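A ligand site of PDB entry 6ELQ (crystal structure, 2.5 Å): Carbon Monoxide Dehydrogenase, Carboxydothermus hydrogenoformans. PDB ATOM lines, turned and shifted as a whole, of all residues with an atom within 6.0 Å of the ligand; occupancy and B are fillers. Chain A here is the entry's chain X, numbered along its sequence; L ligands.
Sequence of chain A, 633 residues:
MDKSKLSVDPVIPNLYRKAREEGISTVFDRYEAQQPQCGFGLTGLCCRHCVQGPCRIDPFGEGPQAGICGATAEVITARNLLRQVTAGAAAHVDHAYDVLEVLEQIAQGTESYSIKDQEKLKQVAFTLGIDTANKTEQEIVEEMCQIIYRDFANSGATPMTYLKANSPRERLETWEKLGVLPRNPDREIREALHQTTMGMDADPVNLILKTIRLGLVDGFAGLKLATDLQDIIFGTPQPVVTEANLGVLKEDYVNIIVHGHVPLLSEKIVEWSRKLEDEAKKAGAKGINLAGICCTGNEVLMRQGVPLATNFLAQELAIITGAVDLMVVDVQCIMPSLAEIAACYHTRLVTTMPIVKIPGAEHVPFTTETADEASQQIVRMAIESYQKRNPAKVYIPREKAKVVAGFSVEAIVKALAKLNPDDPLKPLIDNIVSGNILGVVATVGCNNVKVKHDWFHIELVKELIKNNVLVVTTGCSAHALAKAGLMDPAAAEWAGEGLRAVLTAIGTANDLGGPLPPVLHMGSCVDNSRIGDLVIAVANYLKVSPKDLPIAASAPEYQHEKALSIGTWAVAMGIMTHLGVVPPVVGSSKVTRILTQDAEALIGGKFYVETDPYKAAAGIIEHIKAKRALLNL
SG of Cys 525 is bound to NI1 of the ligand (2.0 Å). An iron atom (FE4) of the ligand is bound by a ring nitrogen (NE2) of His 261 (2.0 Å). FE1 of the ligand is bound by SG of Cys 333, at 2.3 Å. The side-chain sulfur of Cys 295 binds an iron atom (FE4) of the ligand (2.3 Å). The backbone NH (N) of Cys 446 lies close to a sulfur (S1) of the ligand (3.7 Å). An iron atom (FE2) of the ligand is bound by the side-chain sulfur (SG) of Cys 446 (2.3 Å). N of Cys 476 lies close to S1 of the ligand, 3.6 Å away. FE3 of the ligand is bound by SG of Cys 476. NZ of Lys 562 sits close to S4 of the ligand (3.5 Å). NE2 of Gln 559 sits close to S2 of the ligand (3.2 Å). S3 of the ligand lies close to SG of Cys 294 (3.6 Å).
The backbone NH (N) of Cys 525 sits close to the side-chain sulfur (SG) of Cys 295 (3.4 Å). A ring nitrogen (ND1) of His 261 sits close to the backbone carbonyl oxygen (O) of Gln 332 (3.5 Å). The backbone NH (N) of Cys 295 lies within hydrogen-bond range of the backbone carbonyl oxygen (O) of Gly 260 (3.5 Å). The side-chain sulfur of Cys 446 lies close to the backbone NH of Gln 559 (3.3 Å). SG of Cys 446 sits close to N of His 560, 3.6 Å away. The backbone NH (N) of Cys 476 sits at hydrogen-bond distance from the backbone carbonyl oxygen (O) of Gly 445. The side-chain sulfur of Cys 476 sits close to the backbone NH of Phe 312 (3.7 Å). A ring nitrogen (ND1) of His 560 lies within hydrogen-bond range of the backbone NH (N) of Lys 562 (3.0 Å).
A sulfur (S1) of the ligand lies close to the backbone carbonyl oxygen (O) of Gly 445. CB of Phe 312 touches S2 of the ligand, at 3.7 Å. CB of His 560 touches S4 of the ligand, 3.7 Å away. Hydrophobic or aromatic side chains within 4 Å of the ligand: His 261, Phe 312 and His 560. Of the 22 residues printed, 12 come within 4 Å of the ligand.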
ATOM      1  N   HIS A  92     -21.780  10.178  33.131  1.00  0.00           N
ATOM      2  CA  HIS A  92     -22.334   9.292  32.111  1.00  0.00           C
ATOM      3  C   HIS A  92     -22.725   7.940  32.687  1.00  0.00           C
ATOM      4  O   HIS A  92     -23.796   7.415  32.373  1.00  0.00           O
ATOM      5  CB  HIS A  92     -21.338   9.122  30.967  1.00  0.00           C
ATOM      6  CG  HIS A  92     -21.199  10.334  30.103  1.00  0.00           C
ATOM      7  ND1 HIS A  92     -19.980  10.828  29.694  1.00  0.00           N
ATOM      8  CD2 HIS A  92     -22.123  11.165  29.560  1.00  0.00           C
ATOM      9  CE1 HIS A  92     -20.159  11.897  28.942  1.00  0.00           C
ATOM     10  NE2 HIS A  92     -21.454  12.124  28.852  1.00  0.00           N
ATOM     11  N   GLY A 260     -31.884  19.127  29.994  1.00  0.00           N
ATOM     12  CA  GLY A 260     -31.191  18.092  30.743  1.00  0.00           C
ATOM     13  C   GLY A 260     -30.579  17.032  29.854  1.00  0.00           C
ATOM     14  O   GLY A 260     -29.997  17.353  28.819  1.00  0.00           O
ATOM     15  N   HIS A 261     -30.702  15.749  30.231  1.00  0.00           N
ATOM     16  CA  HIS A 261     -29.966  14.726  29.488  1.00  0.00           C
ATOM     17  C   HIS A 261     -30.665  13.375  29.391  1.00  0.00           C
ATOM     18  O   HIS A 261     -30.479  12.655  28.398  1.00  0.00           O
ATOM     19  CB  HIS A 261     -28.580  14.541  30.121  1.00  0.00           C
ATOM     20  CG  HIS A 261     -27.608  15.610  29.740  1.00  0.00           C
ATOM     21  ND1 HIS A 261     -27.631  16.867  30.306  1.00  0.00           N
ATOM     22  CD2 HIS A 261     -26.600  15.611  28.850  1.00  0.00           C
ATOM     23  CE1 HIS A 261     -26.676  17.603  29.772  1.00  0.00           C
ATOM     24  NE2 HIS A 261     -26.037  16.866  28.880  1.00  0.00           N
ATOM     25  N   CYS A 294     -30.255  21.292  25.055  1.00  0.00           N
ATOM     26  CA  CYS A 294     -29.158  20.390  25.421  1.00  0.00           C
ATOM     27  C   CYS A 294     -29.479  18.978  24.942  1.00  0.00           C
ATOM     28  O   CYS A 294     -30.253  18.776  24.000  1.00  0.00           O
ATOM     29  CB  CYS A 294     -28.859  20.493  26.902  1.00  0.00           C
ATOM     30  SG  CYS A 294     -27.756  21.900  27.328  1.00  0.00           S
ATOM     31  N   CYS A 295     -28.897  17.967  25.606  1.00  0.00           N
ATOM     32  CA  CYS A 295     -28.875  16.603  25.084  1.00  0.00           C
ATOM     33  C   CYS A 295     -30.221  15.895  25.158  1.00  0.00           C
ATOM     34  O   CYS A 295     -30.552  15.107  24.265  1.00  0.00           O
ATOM     35  CB  CYS A 295     -27.811  15.777  25.803  1.00  0.00           C
ATOM     36  SG  CYS A 295     -26.149  16.207  25.313  1.00  0.00           S
ATOM     37  N   PHE A 312     -26.318  25.053  25.039  1.00  0.00           N
ATOM     38  CA  PHE A 312     -26.021  25.251  26.457  1.00  0.00           C
ATOM     39  C   PHE A 312     -25.901  26.721  26.826  1.00  0.00           C
ATOM     40  O   PHE A 312     -26.475  27.163  27.835  1.00  0.00           O
ATOM     41  CB  PHE A 312     -24.732  24.505  26.810  1.00  0.00           C
ATOM     42  CG  PHE A 312     -24.096  24.953  28.097  1.00  0.00           C
ATOM     43  CD1 PHE A 312     -24.600  24.524  29.323  1.00  0.00           C
ATOM     44  CD2 PHE A 312     -22.986  25.783  28.090  1.00  0.00           C
ATOM     45  CE1 PHE A 312     -24.011  24.927  30.500  1.00  0.00           C
ATOM     46  CE2 PHE A 312     -22.398  26.194  29.272  1.00  0.00           C
ATOM     47  CZ  PHE A 312     -22.914  25.764  30.480  1.00  0.00           C
ATOM     48  N   GLN A 332     -27.546  17.621  34.945  1.00  0.00           N
ATOM     49  CA  GLN A 332     -26.383  18.028  34.152  1.00  0.00           C
ATOM     50  C   GLN A 332     -26.593  19.287  33.319  1.00  0.00           C
ATOM     51  O   GLN A 332     -27.611  19.449  32.645  1.00  0.00           O
ATOM     52  CB  GLN A 332     -25.940  16.883  33.222  1.00  0.00           C
ATOM     53  CG  GLN A 332     -25.579  15.604  33.941  1.00  0.00           C
ATOM     54  CD  GLN A 332     -25.389  14.441  32.987  1.00  0.00           C
ATOM     55  OE1 GLN A 332     -25.323  14.633  31.772  1.00  0.00           O
ATOM     56  NE2 GLN A 332     -25.316  13.228  33.523  1.00  0.00           N
ATOM     57  N   CYS A 333     -25.607  20.184  33.371  1.00  0.00           N
ATOM     58  CA  CYS A 333     -25.505  21.365  32.503  1.00  0.00           C
ATOM     59  C   CYS A 333     -26.660  22.334  32.684  1.00  0.00           C
ATOM     60  O   CYS A 333     -26.895  23.187  31.830  1.00  0.00           O
ATOM     61  CB  CYS A 333     -25.394  20.948  31.033  1.00  0.00           C
ATOM     62  SG  CYS A 333     -23.961  19.905  30.698  1.00  0.00           S
ATOM     63  N   GLY A 445     -19.262  18.262  21.770  1.00  0.00           N
ATOM     64  CA  GLY A 445     -18.996  19.130  22.896  1.00  0.00           C
ATOM     65  C   GLY A 445     -20.065  20.180  23.098  1.00  0.00           C
ATOM     66  O   GLY A 445     -21.106  20.206  22.448  1.00  0.00           O
ATOM     67  N   CYS A 446     -19.770  21.077  24.035  1.00  0.00           N
ATOM     68  CA  CYS A 446     -20.719  22.034  24.560  1.00  0.00           C
ATOM     69  C   CYS A 446     -20.439  23.434  24.003  1.00  0.00           C
ATOM     70  O   CYS A 446     -19.791  23.579  22.953  1.00  0.00           O
ATOM     71  CB  CYS A 446     -20.647  22.000  26.086  1.00  0.00           C
ATOM     72  SG  CYS A 446     -19.567  20.702  26.768  1.00  0.00           S
ATOM     73  N   ASN A 447     -20.945  24.450  24.692  1.00  0.00           N
ATOM     74  CA  ASN A 447     -20.552  25.834  24.470  1.00  0.00           C
ATOM     75  C   ASN A 447     -19.675  26.297  25.624  1.00  0.00           C
ATOM     76  O   ASN A 447     -19.802  25.822  26.757  1.00  0.00           O
ATOM     77  CB  ASN A 447     -21.764  26.757  24.366  1.00  0.00           C
ATOM     78  CG  ASN A 447     -22.641  26.448  23.175  1.00  0.00           C
ATOM     79  OD1 ASN A 447     -23.852  26.291  23.312  1.00  0.00           O
ATOM     80  ND2 ASN A 447     -22.034  26.351  21.995  1.00  0.00           N
ATOM     81  N   THR A 474     -22.831  15.689  17.510  1.00  0.00           N
ATOM     82  CA  THR A 474     -23.689  15.368  18.646  1.00  0.00           C
ATOM     83  C   THR A 474     -23.696  16.560  19.601  1.00  0.00           C
ATOM     84  O   THR A 474     -22.979  17.542  19.397  1.00  0.00           O
ATOM     85  CB  THR A 474     -23.216  14.107  19.376  1.00  0.00           C
ATOM     86  OG1 THR A 474     -21.826  14.218  19.690  1.00  0.00           O
ATOM     87  CG2 THR A 474     -23.441  12.844  18.549  1.00  0.00           C
ATOM     88  N   GLY A 475     -24.515  16.457  20.641  1.00  0.00           N
ATOM     89  CA  GLY A 475     -24.495  17.396  21.744  1.00  0.00           C
ATOM     90  C   GLY A 475     -24.816  18.818  21.328  1.00  0.00           C
ATOM     91  O   GLY A 475     -25.604  19.080  20.417  1.00  0.00           O
ATOM     92  N   CYS A 476     -24.198  19.773  22.030  1.00  0.00           N
ATOM     93  CA  CYS A 476     -24.429  21.184  21.744  1.00  0.00           C
ATOM     94  C   CYS A 476     -23.725  21.645  20.485  1.00  0.00           C
ATOM     95  O   CYS A 476     -24.157  22.627  19.876  1.00  0.00           O
ATOM     96  CB  CYS A 476     -24.001  22.040  22.937  1.00  0.00           C
ATOM     97  SG  CYS A 476     -24.928  21.695  24.449  1.00  0.00           S
ATOM     98  N   SER A 477     -22.658  20.956  20.064  1.00  0.00           N
ATOM     99  CA  SER A 477     -22.112  21.193  18.733  1.00  0.00           C
ATOM    100  C   SER A 477     -23.144  20.928  17.656  1.00  0.00           C
ATOM    101  O   SER A 477     -23.161  21.610  16.623  1.00  0.00           O
ATOM    102  CB  SER A 477     -20.876  20.324  18.510  1.00  0.00           C
ATOM    103  OG  SER A 477     -20.385  20.453  17.173  1.00  0.00           O
ATOM    104  N   CYS A 525     -24.948  13.570  23.616  1.00  0.00           N
ATOM    105  CA  CYS A 525     -23.569  13.322  24.056  1.00  0.00           C
ATOM    106  C   CYS A 525     -23.297  11.827  24.211  1.00  0.00           C
ATOM    107  O   CYS A 525     -22.260  11.332  23.773  1.00  0.00           O
ATOM    108  CB  CYS A 525     -23.301  14.066  25.371  1.00  0.00           C
ATOM    109  SG  CYS A 525     -22.709  15.788  25.215  1.00  0.00           S
ATOM    110  N   VAL A 526     -24.234  11.102  24.840  1.00  0.00           N
ATOM    111  CA  VAL A 526     -24.059   9.653  24.952  1.00  0.00           C
ATOM    112  C   VAL A 526     -24.056   9.000  23.583  1.00  0.00           C
ATOM    113  O   VAL A 526     -23.401   7.970  23.378  1.00  0.00           O
ATOM    114  CB  VAL A 526     -25.159   9.050  25.863  1.00  0.00           C
ATOM    115  CG1 VAL A 526     -25.023   9.573  27.284  1.00  0.00           C
ATOM    116  CG2 VAL A 526     -26.539   9.326  25.314  1.00  0.00           C
ATOM    117  N   GLN A 559     -16.906  22.511  27.680  1.00  0.00           N
ATOM    118  CA  GLN A 559     -16.864  23.135  29.001  1.00  0.00           C
ATOM    119  C   GLN A 559     -16.993  22.102  30.124  1.00  0.00           C
ATOM    120  O   GLN A 559     -16.294  22.201  31.132  1.00  0.00           O
ATOM    121  CB  GLN A 559     -17.958  24.198  29.142  1.00  0.00           C
ATOM    122  CG  GLN A 559     -19.392  23.695  28.974  1.00  0.00           C
ATOM    123  CD  GLN A 559     -20.045  23.325  30.297  1.00  0.00           C
ATOM    124  OE1 GLN A 559     -19.480  23.546  31.370  1.00  0.00           O
ATOM    125  NE2 GLN A 559     -21.248  22.760  30.219  1.00  0.00           N
ATOM    126  N   HIS A 560     -17.857  21.114  29.943  1.00  0.00           N
ATOM    127  CA  HIS A 560     -18.189  20.196  31.032  1.00  0.00           C
ATOM    128  C   HIS A 560     -17.119  19.113  31.172  1.00  0.00           C
ATOM    129  O   HIS A 560     -16.446  18.737  30.208  1.00  0.00           O
ATOM    130  CB  HIS A 560     -19.548  19.549  30.775  1.00  0.00           C
ATOM    131  CG  HIS A 560     -20.208  19.012  32.013  1.00  0.00           C
ATOM    132  ND1 HIS A 560     -19.952  17.754  32.514  1.00  0.00           N
ATOM    133  CD2 HIS A 560     -21.116  19.573  32.853  1.00  0.00           C
ATOM    134  CE1 HIS A 560     -20.673  17.551  33.601  1.00  0.00           C
ATOM    135  NE2 HIS A 560     -21.391  18.641  33.826  1.00  0.00           N
ATOM    136  N   LYS A 562     -17.711  16.145  31.416  1.00  0.00           N
ATOM    137  CA  LYS A 562     -18.100  15.054  30.524  1.00  0.00           C
ATOM    138  C   LYS A 562     -17.373  15.139  29.202  1.00  0.00           C
ATOM    139  O   LYS A 562     -17.101  14.109  28.577  1.00  0.00           O
ATOM    140  CB  LYS A 562     -19.613  15.052  30.316  1.00  0.00           C
ATOM    141  CG  LYS A 562     -20.417  14.541  31.506  1.00  0.00           C
ATOM    142  CD  LYS A 562     -21.908  14.588  31.220  1.00  0.00           C
ATOM    143  CE  LYS A 562     -22.399  16.026  31.124  1.00  0.00           C
ATOM    144  NZ  LYS A 562     -23.805  16.141  30.668  1.00  0.00           N
ATOM    145  N   ALA A 563     -17.037  16.353  28.746  1.00  0.00           N
ATOM    146  CA  ALA A 563     -16.317  16.490  27.488  1.00  0.00           C
ATOM    147  C   ALA A 563     -14.868  16.044  27.618  1.00  0.00           C
ATOM    148  O   ALA A 563     -14.313  15.462  26.674  1.00  0.00           O
ATOM    149  CB  ALA A 563     -16.389  17.936  26.997  1.00  0.00           C
ATOM    150  N   ILE A 566     -15.058  12.278  27.375  1.00  0.00           N
ATOM    151  CA  ILE A 566     -15.317  11.875  25.992  1.00  0.00           C
ATOM    152  C   ILE A 566     -14.080  12.084  25.133  1.00  0.00           C
ATOM    153  O   ILE A 566     -13.695  11.210  24.347  1.00  0.00           O
ATOM    154  CB  ILE A 566     -16.526  12.648  25.438  1.00  0.00           C
ATOM    155  CG1 ILE A 566     -17.809  12.221  26.167  1.00  0.00           C
ATOM    156  CG2 ILE A 566     -16.661  12.431  23.942  1.00  0.00           C
ATOM    157  CD1 ILE A 566     -18.992  13.084  25.861  1.00  0.00           C
HETATM  158  O1  LIG L   1     -23.729  15.813  27.937  1.00  0.00           O
HETATM  159  S1  LIG L   1     -22.607  18.953  25.148  1.00  0.00           S
HETATM  160  S2  LIG L   1     -22.731  21.545  27.620  1.00  0.00           S
HETATM  161  S3  LIG L   1     -25.375  19.261  27.402  1.00  0.00           S
HETATM  162  S4  LIG L   1     -21.935  18.004  28.391  1.00  0.00           S
HETATM  163 FE1  LIG L   1     -23.516  19.661  28.474  1.00  0.00          FE
HETATM  164 FE2  LIG L   1     -21.631  19.720  26.989  1.00  0.00          FE
HETATM  165 FE3  LIG L   1     -23.916  20.416  26.089  1.00  0.00          FE
HETATM  166 FE4  LIG L   1     -25.062  17.116  27.115  1.00  0.00          FE
HETATM  167 NI1  LIG L   1     -21.943  17.093  26.541  1.00  0.00          NI
